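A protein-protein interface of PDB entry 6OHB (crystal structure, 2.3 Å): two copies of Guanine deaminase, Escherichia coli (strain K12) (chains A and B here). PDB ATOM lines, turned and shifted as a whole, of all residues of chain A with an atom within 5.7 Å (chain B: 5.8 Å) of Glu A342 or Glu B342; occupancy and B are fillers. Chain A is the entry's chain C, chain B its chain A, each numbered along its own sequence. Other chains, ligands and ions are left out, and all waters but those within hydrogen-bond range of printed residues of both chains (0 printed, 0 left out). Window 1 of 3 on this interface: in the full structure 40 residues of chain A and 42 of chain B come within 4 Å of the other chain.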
ATOM      1  N   PRO A 299       5.354 -35.851  28.658  1.00  0.00           N
ATOM      2  CA  PRO A 299       6.160 -34.820  27.989  1.00  0.00           C
ATOM      3  C   PRO A 299       6.625 -33.701  28.912  1.00  0.00           C
ATOM      4  O   PRO A 299       7.746 -33.192  28.743  1.00  0.00           O
ATOM      5  CB  PRO A 299       5.231 -34.302  26.887  1.00  0.00           C
ATOM      6  CG  PRO A 299       3.876 -34.562  27.394  1.00  0.00           C
ATOM      7  CD  PRO A 299       3.960 -35.854  28.183  1.00  0.00           C
ATOM      8  N   THR A 300       5.797 -33.301  29.881  1.00  0.00           N
ATOM      9  CA  THR A 300       6.107 -32.124  30.693  1.00  0.00           C
ATOM     10  C   THR A 300       7.360 -32.335  31.535  1.00  0.00           C
ATOM     11  O   THR A 300       8.275 -31.503  31.524  1.00  0.00           O
ATOM     12  CB  THR A 300       4.915 -31.762  31.586  1.00  0.00           C
ATOM     13  OG1 THR A 300       3.715 -31.748  30.805  1.00  0.00           O
ATOM     14  CG2 THR A 300       5.122 -30.390  32.232  1.00  0.00           C
ATOM     15  N   LEU A 303      10.471 -32.397  29.504  1.00  0.00           N
ATOM     16  CA  LEU A 303      10.978 -31.068  29.181  1.00  0.00           C
ATOM     17  C   LEU A 303      11.664 -30.422  30.384  1.00  0.00           C
ATOM     18  O   LEU A 303      12.808 -29.961  30.279  1.00  0.00           O
ATOM     19  CB  LEU A 303       9.842 -30.186  28.672  1.00  0.00           C
ATOM     20  CG  LEU A 303       9.355 -30.507  27.262  1.00  0.00           C
ATOM     21  CD1 LEU A 303       8.230 -29.564  26.846  1.00  0.00           C
ATOM     22  CD2 LEU A 303      10.515 -30.441  26.290  1.00  0.00           C
ATOM     23  N   LEU A 337      -5.332 -31.675  29.621  1.00  0.00           N
ATOM     24  CA  LEU A 337      -5.296 -30.797  28.450  1.00  0.00           C
ATOM     25  C   LEU A 337      -3.924 -30.150  28.294  1.00  0.00           C
ATOM     26  O   LEU A 337      -3.354 -30.126  27.195  1.00  0.00           O
ATOM     27  CB  LEU A 337      -6.385 -29.728  28.546  1.00  0.00           C
ATOM     28  CG  LEU A 337      -7.834 -30.181  28.701  1.00  0.00           C
ATOM     29  CD1 LEU A 337      -8.730 -28.973  28.958  1.00  0.00           C
ATOM     30  CD2 LEU A 337      -8.292 -30.955  27.473  1.00  0.00           C
ATOM     31  N   GLN A 338      -3.376 -29.612  29.388  1.00  0.00           N
ATOM     32  CA  GLN A 338      -2.045 -29.014  29.322  1.00  0.00           C
ATOM     33  C   GLN A 338      -0.980 -30.063  29.020  1.00  0.00           C
ATOM     34  O   GLN A 338      -0.017 -29.785  28.296  1.00  0.00           O
ATOM     35  CB  GLN A 338      -1.732 -28.278  30.625  1.00  0.00           C
ATOM     36  CG  GLN A 338      -2.759 -27.204  30.980  1.00  0.00           C
ATOM     37  CD  GLN A 338      -2.319 -26.334  32.140  1.00  0.00           C
ATOM     38  OE1 GLN A 338      -2.064 -26.829  33.240  1.00  0.00           O
ATOM     39  NE2 GLN A 338      -2.230 -25.029  31.903  1.00  0.00           N
ATOM     40  N   THR A 339      -1.137 -31.279  29.553  1.00  0.00           N
ATOM     41  CA  THR A 339      -0.219 -32.363  29.204  1.00  0.00           C
ATOM     42  C   THR A 339      -0.221 -32.626  27.700  1.00  0.00           C
ATOM     43  O   THR A 339       0.838 -32.823  27.091  1.00  0.00           O
ATOM     44  CB  THR A 339      -0.586 -33.633  29.968  1.00  0.00           C
ATOM     45  OG1 THR A 339      -0.493 -33.388  31.376  1.00  0.00           O
ATOM     46  CG2 THR A 339       0.358 -34.756  29.598  1.00  0.00           C
ATOM     47  N   LEU A 340      -1.401 -32.634  27.079  1.00  0.00           N
ATOM     48  CA  LEU A 340      -1.456 -32.858  25.637  1.00  0.00           C
ATOM     49  C   LEU A 340      -0.893 -31.677  24.862  1.00  0.00           C
ATOM     50  O   LEU A 340      -0.297 -31.859  23.795  1.00  0.00           O
ATOM     51  CB  LEU A 340      -2.892 -33.135  25.201  1.00  0.00           C
ATOM     52  CG  LEU A 340      -3.477 -34.433  25.744  1.00  0.00           C
ATOM     53  CD1 LEU A 340      -4.979 -34.416  25.569  1.00  0.00           C
ATOM     54  CD2 LEU A 340      -2.852 -35.614  25.032  1.00  0.00           C
ATOM     55  N   ASN A 341      -1.073 -30.462  25.376  1.00  0.00           N
ATOM     56  CA  ASN A 341      -0.421 -29.307  24.764  1.00  0.00           C
ATOM     57  C   ASN A 341       1.098 -29.469  24.755  1.00  0.00           C
ATOM     58  O   ASN A 341       1.763 -29.236  23.730  1.00  0.00           O
ATOM     59  CB  ASN A 341      -0.825 -28.040  25.506  1.00  0.00           C
ATOM     60  CG  ASN A 341      -0.792 -26.827  24.619  1.00  0.00           C
ATOM     61  OD1 ASN A 341      -1.121 -26.906  23.434  1.00  0.00           O
ATOM     62  ND2 ASN A 341      -0.377 -25.698  25.176  1.00  0.00           N
ATOM     63  N   GLU A 342       1.668 -29.898  25.887  1.00  0.00           N
ATOM     64  CA  GLU A 342       3.119 -30.081  25.934  1.00  0.00           C
ATOM     65  C   GLU A 342       3.548 -31.227  25.025  1.00  0.00           C
ATOM     66  O   GLU A 342       4.619 -31.168  24.410  1.00  0.00           O
ATOM     67  CB  GLU A 342       3.616 -30.323  27.362  1.00  0.00           C
ATOM     68  CG  GLU A 342       2.937 -29.499  28.463  1.00  0.00           C
ATOM     69  CD  GLU A 342       2.943 -27.989  28.220  1.00  0.00           C
ATOM     70  OE1 GLU A 342       1.900 -27.343  28.497  1.00  0.00           O
ATOM     71  OE2 GLU A 342       3.985 -27.450  27.780  1.00  0.00           O
ATOM     72  N   ALA A 343       2.732 -32.283  24.937  1.00  0.00           N
ATOM     73  CA  ALA A 343       3.012 -33.352  23.982  1.00  0.00           C
ATOM     74  C   ALA A 343       3.030 -32.817  22.555  1.00  0.00           C
ATOM     75  O   ALA A 343       3.889 -33.198  21.752  1.00  0.00           O
ATOM     76  CB  ALA A 343       1.979 -34.474  24.124  1.00  0.00           C
ATOM     77  N   TYR A 344       2.086 -31.932  22.222  1.00  0.00           N
ATOM     78  CA  TYR A 344       2.060 -31.328  20.893  1.00  0.00           C
ATOM     79  C   TYR A 344       3.358 -30.581  20.607  1.00  0.00           C
ATOM     80  O   TYR A 344       3.930 -30.708  19.520  1.00  0.00           O
ATOM     81  CB  TYR A 344       0.852 -30.393  20.777  1.00  0.00           C
ATOM     82  CG  TYR A 344       0.732 -29.664  19.454  1.00  0.00           C
ATOM     83  CD1 TYR A 344       0.088 -30.250  18.367  1.00  0.00           C
ATOM     84  CD2 TYR A 344       1.253 -28.383  19.293  1.00  0.00           C
ATOM     85  CE1 TYR A 344      -0.027 -29.586  17.154  1.00  0.00           C
ATOM     86  CE2 TYR A 344       1.145 -27.706  18.082  1.00  0.00           C
ATOM     87  CZ  TYR A 344       0.504 -28.314  17.018  1.00  0.00           C
ATOM     88  OH  TYR A 344       0.397 -27.643  15.820  1.00  0.00           O
ATOM     89  N   LYS A 345       3.857 -29.822  21.589  1.00  0.00           N
ATOM     90  CA  LYS A 345       5.129 -29.115  21.389  1.00  0.00           C
ATOM     91  C   LYS A 345       6.302 -30.088  21.236  1.00  0.00           C
ATOM     92  O   LYS A 345       7.156 -29.919  20.345  1.00  0.00           O
ATOM     93  CB  LYS A 345       5.379 -28.151  22.549  1.00  0.00           C
ATOM     94  CG  LYS A 345       4.343 -27.040  22.652  1.00  0.00           C
ATOM     95  CD  LYS A 345       4.572 -26.180  23.882  1.00  0.00           C
ATOM     96  CE  LYS A 345       3.268 -25.873  24.594  1.00  0.00           C
ATOM     97  NZ  LYS A 345       3.495 -25.611  26.047  1.00  0.00           N
ATOM     98  N   VAL A 346       6.348 -31.119  22.088  1.00  0.00           N
ATOM     99  CA  VAL A 346       7.421 -32.111  22.041  1.00  0.00           C
ATOM    100  C   VAL A 346       7.471 -32.779  20.673  1.00  0.00           C
ATOM    101  O   VAL A 346       8.550 -33.014  20.113  1.00  0.00           O
ATOM    102  CB  VAL A 346       7.231 -33.144  23.171  1.00  0.00           C
ATOM    103  CG1 VAL A 346       8.003 -34.430  22.884  1.00  0.00           C
ATOM    104  CG2 VAL A 346       7.653 -32.556  24.517  1.00  0.00           C
ATOM    105  N   LEU A 347       6.303 -33.124  20.125  1.00  0.00           N
ATOM    106  CA  LEU A 347       6.238 -33.783  18.827  1.00  0.00           C
ATOM    107  C   LEU A 347       6.501 -32.818  17.673  1.00  0.00           C
ATOM    108  O   LEU A 347       7.071 -33.221  16.652  1.00  0.00           O
ATOM    109  CB  LEU A 347       4.886 -34.481  18.682  1.00  0.00           C
ATOM    110  CG  LEU A 347       4.784 -35.532  19.791  1.00  0.00           C
ATOM    111  CD1 LEU A 347       3.348 -35.996  20.005  1.00  0.00           C
ATOM    112  CD2 LEU A 347       5.722 -36.711  19.514  1.00  0.00           C
ATOM    113  N   PRO B 299       9.381 -18.028  23.291  1.00  0.00           N
ATOM    114  CA  PRO B 299       9.486 -19.498  23.299  1.00  0.00           C
ATOM    115  C   PRO B 299       8.209 -20.218  22.879  1.00  0.00           C
ATOM    116  O   PRO B 299       8.285 -21.270  22.222  1.00  0.00           O
ATOM    117  CB  PRO B 299       9.871 -19.814  24.749  1.00  0.00           C
ATOM    118  CG  PRO B 299       9.406 -18.625  25.535  1.00  0.00           C
ATOM    119  CD  PRO B 299       9.598 -17.445  24.625  1.00  0.00           C
ATOM    120  N   THR B 300       7.036 -19.681  23.223  1.00  0.00           N
ATOM    121  CA  THR B 300       5.788 -20.408  23.000  1.00  0.00           C
ATOM    122  C   THR B 300       5.518 -20.625  21.514  1.00  0.00           C
ATOM    123  O   THR B 300       5.267 -21.756  21.077  1.00  0.00           O
ATOM    124  CB  THR B 300       4.625 -19.656  23.656  1.00  0.00           C
ATOM    125  OG1 THR B 300       4.865 -19.540  25.060  1.00  0.00           O
ATOM    126  CG2 THR B 300       3.314 -20.399  23.440  1.00  0.00           C
ATOM    127  N   LEU B 303       7.916 -23.009  19.859  1.00  0.00           N
ATOM    128  CA  LEU B 303       7.632 -24.426  20.053  1.00  0.00           C
ATOM    129  C   LEU B 303       6.408 -24.880  19.255  1.00  0.00           C
ATOM    130  O   LEU B 303       6.435 -25.953  18.641  1.00  0.00           O
ATOM    131  CB  LEU B 303       7.447 -24.725  21.539  1.00  0.00           C
ATOM    132  CG  LEU B 303       8.723 -24.765  22.382  1.00  0.00           C
ATOM    133  CD1 LEU B 303       8.392 -25.036  23.840  1.00  0.00           C
ATOM    134  CD2 LEU B 303       9.681 -25.811  21.842  1.00  0.00           C
ATOM    135  N   LEU B 337       4.268 -14.933  32.950  1.00  0.00           N
ATOM    136  CA  LEU B 337       4.734 -16.048  33.772  1.00  0.00           C
ATOM    137  C   LEU B 337       4.779 -17.336  32.960  1.00  0.00           C
ATOM    138  O   LEU B 337       5.763 -18.085  33.009  1.00  0.00           O
ATOM    139  CB  LEU B 337       3.850 -16.205  35.014  1.00  0.00           C
ATOM    140  CG  LEU B 337       3.735 -14.989  35.941  1.00  0.00           C
ATOM    141  CD1 LEU B 337       2.718 -15.253  37.042  1.00  0.00           C
ATOM    142  CD2 LEU B 337       5.086 -14.628  36.534  1.00  0.00           C
ATOM    143  N   GLN B 338       3.712 -17.607  32.206  1.00  0.00           N
ATOM    144  CA  GLN B 338       3.682 -18.787  31.352  1.00  0.00           C
ATOM    145  C   GLN B 338       4.718 -18.695  30.237  1.00  0.00           C
ATOM    146  O   GLN B 338       5.320 -19.711  29.857  1.00  0.00           O
ATOM    147  CB  GLN B 338       2.274 -18.967  30.780  1.00  0.00           C
ATOM    148  CG  GLN B 338       1.221 -19.156  31.860  1.00  0.00           C
ATOM    149  CD  GLN B 338      -0.162 -19.417  31.304  1.00  0.00           C
ATOM    150  OE1 GLN B 338      -0.752 -18.560  30.647  1.00  0.00           O
ATOM    151  NE2 GLN B 338      -0.692 -20.605  31.571  1.00  0.00           N
ATOM    152  N   THR B 339       4.947 -17.487  29.703  1.00  0.00           N
ATOM    153  CA  THR B 339       6.000 -17.305  28.703  1.00  0.00           C
ATOM    154  C   THR B 339       7.362 -17.695  29.263  1.00  0.00           C
ATOM    155  O   THR B 339       8.159 -18.362  28.587  1.00  0.00           O
ATOM    156  CB  THR B 339       6.025 -15.860  28.200  1.00  0.00           C
ATOM    157  OG1 THR B 339       4.742 -15.519  27.667  1.00  0.00           O
ATOM    158  CG2 THR B 339       7.072 -15.688  27.112  1.00  0.00           C
ATOM    159  N   LEU B 340       7.649 -17.291  30.499  1.00  0.00           N
ATOM    160  CA  LEU B 340       8.920 -17.658  31.108  1.00  0.00           C
ATOM    161  C   LEU B 340       8.970 -19.149  31.414  1.00  0.00           C
ATOM    162  O   LEU B 340      10.039 -19.758  31.344  1.00  0.00           O
ATOM    163  CB  LEU B 340       9.149 -16.839  32.376  1.00  0.00           C
ATOM    164  CG  LEU B 340       9.290 -15.329  32.193  1.00  0.00           C
ATOM    165  CD1 LEU B 340       9.155 -14.630  33.541  1.00  0.00           C
ATOM    166  CD2 LEU B 340      10.616 -14.980  31.524  1.00  0.00           C
ATOM    167  N   ASN B 341       7.831 -19.752  31.751  1.00  0.00           N
ATOM    168  CA  ASN B 341       7.784 -21.210  31.878  1.00  0.00           C
ATOM    169  C   ASN B 341       8.210 -21.895  30.578  1.00  0.00           C
ATOM    170  O   ASN B 341       9.014 -22.847  30.586  1.00  0.00           O
ATOM    171  CB  ASN B 341       6.375 -21.643  32.277  1.00  0.00           C
ATOM    172  CG  ASN B 341       6.345 -23.013  32.919  1.00  0.00           C
ATOM    173  OD1 ASN B 341       7.230 -23.369  33.697  1.00  0.00           O
ATOM    174  ND2 ASN B 341       5.322 -23.796  32.591  1.00  0.00           N
ATOM    175  N   GLU B 342       7.701 -21.407  29.442  1.00  0.00           N
ATOM    176  CA  GLU B 342       8.081 -22.005  28.162  1.00  0.00           C
ATOM    177  C   GLU B 342       9.551 -21.754  27.848  1.00  0.00           C
ATOM    178  O   GLU B 342      10.239 -22.635  27.313  1.00  0.00           O
ATOM    179  CB  GLU B 342       7.196 -21.470  27.036  1.00  0.00           C
ATOM    180  CG  GLU B 342       5.718 -21.767  27.214  1.00  0.00           C
ATOM    181  CD  GLU B 342       5.404 -23.250  27.151  1.00  0.00           C
ATOM    182  OE1 GLU B 342       5.931 -23.930  26.244  1.00  0.00           O
ATOM    183  OE2 GLU B 342       4.628 -23.732  28.005  1.00  0.00           O
ATOM    184  N   ALA B 343      10.048 -20.561  28.183  1.00  0.00           N
ATOM    185  CA  ALA B 343      11.470 -20.279  28.014  1.00  0.00           C
ATOM    186  C   ALA B 343      12.314 -21.235  28.839  1.00  0.00           C
ATOM    187  O   ALA B 343      13.360 -21.713  28.380  1.00  0.00           O
ATOM    188  CB  ALA B 343      11.773 -18.832  28.399  1.00  0.00           C
ATOM    189  N   TYR B 344      11.878 -21.517  30.067  1.00  0.00           N
ATOM    190  CA  TYR B 344      12.588 -22.466  30.914  1.00  0.00           C
ATOM    191  C   TYR B 344      12.647 -23.848  30.267  1.00  0.00           C
ATOM    192  O   TYR B 344      13.693 -24.511  30.299  1.00  0.00           O
ATOM    193  CB  TYR B 344      11.919 -22.529  32.289  1.00  0.00           C
ATOM    194  CG  TYR B 344      12.617 -23.448  33.263  1.00  0.00           C
ATOM    195  CD1 TYR B 344      12.311 -24.810  33.313  1.00  0.00           C
ATOM    196  CD2 TYR B 344      13.587 -22.961  34.130  1.00  0.00           C
ATOM    197  CE1 TYR B 344      12.956 -25.659  34.203  1.00  0.00           C
ATOM    198  CE2 TYR B 344      14.236 -23.799  35.023  1.00  0.00           C
ATOM    199  CZ  TYR B 344      13.918 -25.145  35.055  1.00  0.00           C
ATOM    200  OH  TYR B 344      14.563 -25.976  35.944  1.00  0.00           O
ATOM    201  N   LYS B 345      11.539 -24.307  29.673  1.00  0.00           N
ATOM    202  CA  LYS B 345      11.588 -25.618  29.009  1.00  0.00           C
ATOM    203  C   LYS B 345      12.517 -25.601  27.793  1.00  0.00           C
ATOM    204  O   LYS B 345      13.302 -26.538  27.588  1.00  0.00           O
ATOM    205  CB  LYS B 345      10.188 -26.089  28.611  1.00  0.00           C
ATOM    206  CG  LYS B 345       9.285 -26.398  29.796  1.00  0.00           C
ATOM    207  CD  LYS B 345       7.877 -26.704  29.332  1.00  0.00           C
ATOM    208  CE  LYS B 345       6.846 -25.974  30.163  1.00  0.00           C
ATOM    209  NZ  LYS B 345       5.628 -25.697  29.357  1.00  0.00           N
ATOM    210  N   VAL B 346      12.446 -24.546  26.978  1.00  0.00           N
ATOM    211  CA  VAL B 346      13.320 -24.444  25.808  1.00  0.00           C
ATOM    212  C   VAL B 346      14.790 -24.499  26.231  1.00  0.00           C
ATOM    213  O   VAL B 346      15.612 -25.229  25.644  1.00  0.00           O
ATOM    214  CB  VAL B 346      12.997 -23.144  25.042  1.00  0.00           C
ATOM    215  CG1 VAL B 346      14.183 -22.688  24.206  1.00  0.00           C
ATOM    216  CG2 VAL B 346      11.747 -23.318  24.184  1.00  0.00           C
ATOM    217  N   LEU B 347      15.131 -23.772  27.294  1.00  0.00           N
ATOM    218  CA  LEU B 347      16.523 -23.720  27.721  1.00  0.00           C
ATOM    219  C   LEU B 347      16.956 -25.025  28.379  1.00  0.00           C
ATOM    220  O   LEU B 347      18.108 -25.447  28.219  1.00  0.00           O
ATOM    221  CB  LEU B 347      16.724 -22.517  28.639  1.00  0.00           C
ATOM    222  CG  LEU B 347      16.482 -21.289  27.760  1.00  0.00           C
ATOM    223  CD1 LEU B 347      16.221 -20.032  28.578  1.00  0.00           C
ATOM    224  CD2 LEU B 347      17.642 -21.103  26.781  1.00  0.00           C
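The side-chain carboxylate (OE2) of Glu B342 is in salt-bridge range of the side-chain amino group (NZ) of Lys A345 (2.9 Å).
The side-chain carboxylate of Glu A342 lies within salt-bridge range of the side-chain amino group of Lys B345, at 2.9 Å.
The side-chain carboxylate of Glu B342 lies within salt-bridge range of the side-chain amino group of Lys B345, at 2.6 Å.
The side-chain amino group (NZ) of Lys A345 is in salt-bridge range of the side-chain carboxylate (OE2) of Glu A342 (2.6 Å).
Lys B345 touches Leu A303 (CD to CD1, 3.8 Å).
OE2 of Glu B342 touches OE2 of Glu A342, at 3.8 Å.
Lys A345 touches Leu B303.
Lys B345 touches Lys A345.
Hydrophobic or aromatic side chains of chain A that line the printed part of chain B: Leu A303.
Of the 14 printed residues of chain B, 3 touch a printed residue of chain A.
Printed residues of chain B that touch a printed residue of chain A: Leu B303, Glu B342 and Lys B345.
Hydrophobic or aromatic side chains of chain B within 4 Å of the printed part of chain A: Leu B303.
Among the printed residues, 6 pairs touch across the chains.
Glu A342 touches just these residues of chain B: Glu B342 and Lys B345.
Of chain A, only Glu A342 (3.8 Å) and Lys A345 (2.9 Å) come within 4 Å of Glu B342.
Of the printed residues of chain A, Leu B303 touches Lys A345.
Of the printed residues of chain B, Leu A303 touches Lys B345 (3.8 Å).
Thr B339 touches none of the printed residues of chain A.
Ala B343 touches none of the printed residues of chain A.
Leu A303 touches Lys B345, and with the chains exchanged Lys A345 touches Leu B303.
Glu A342 touches its own counterpart, Glu B342.
Glu A342 touches Lys B345, and with the chains exchanged Lys A345 touches Glu B342.
Lys A345 touches its own counterpart, Lys B345.
Of the 6 pairs that touch across the chains among the printed residues, 6 have their exchanged pair printed and touching as well.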
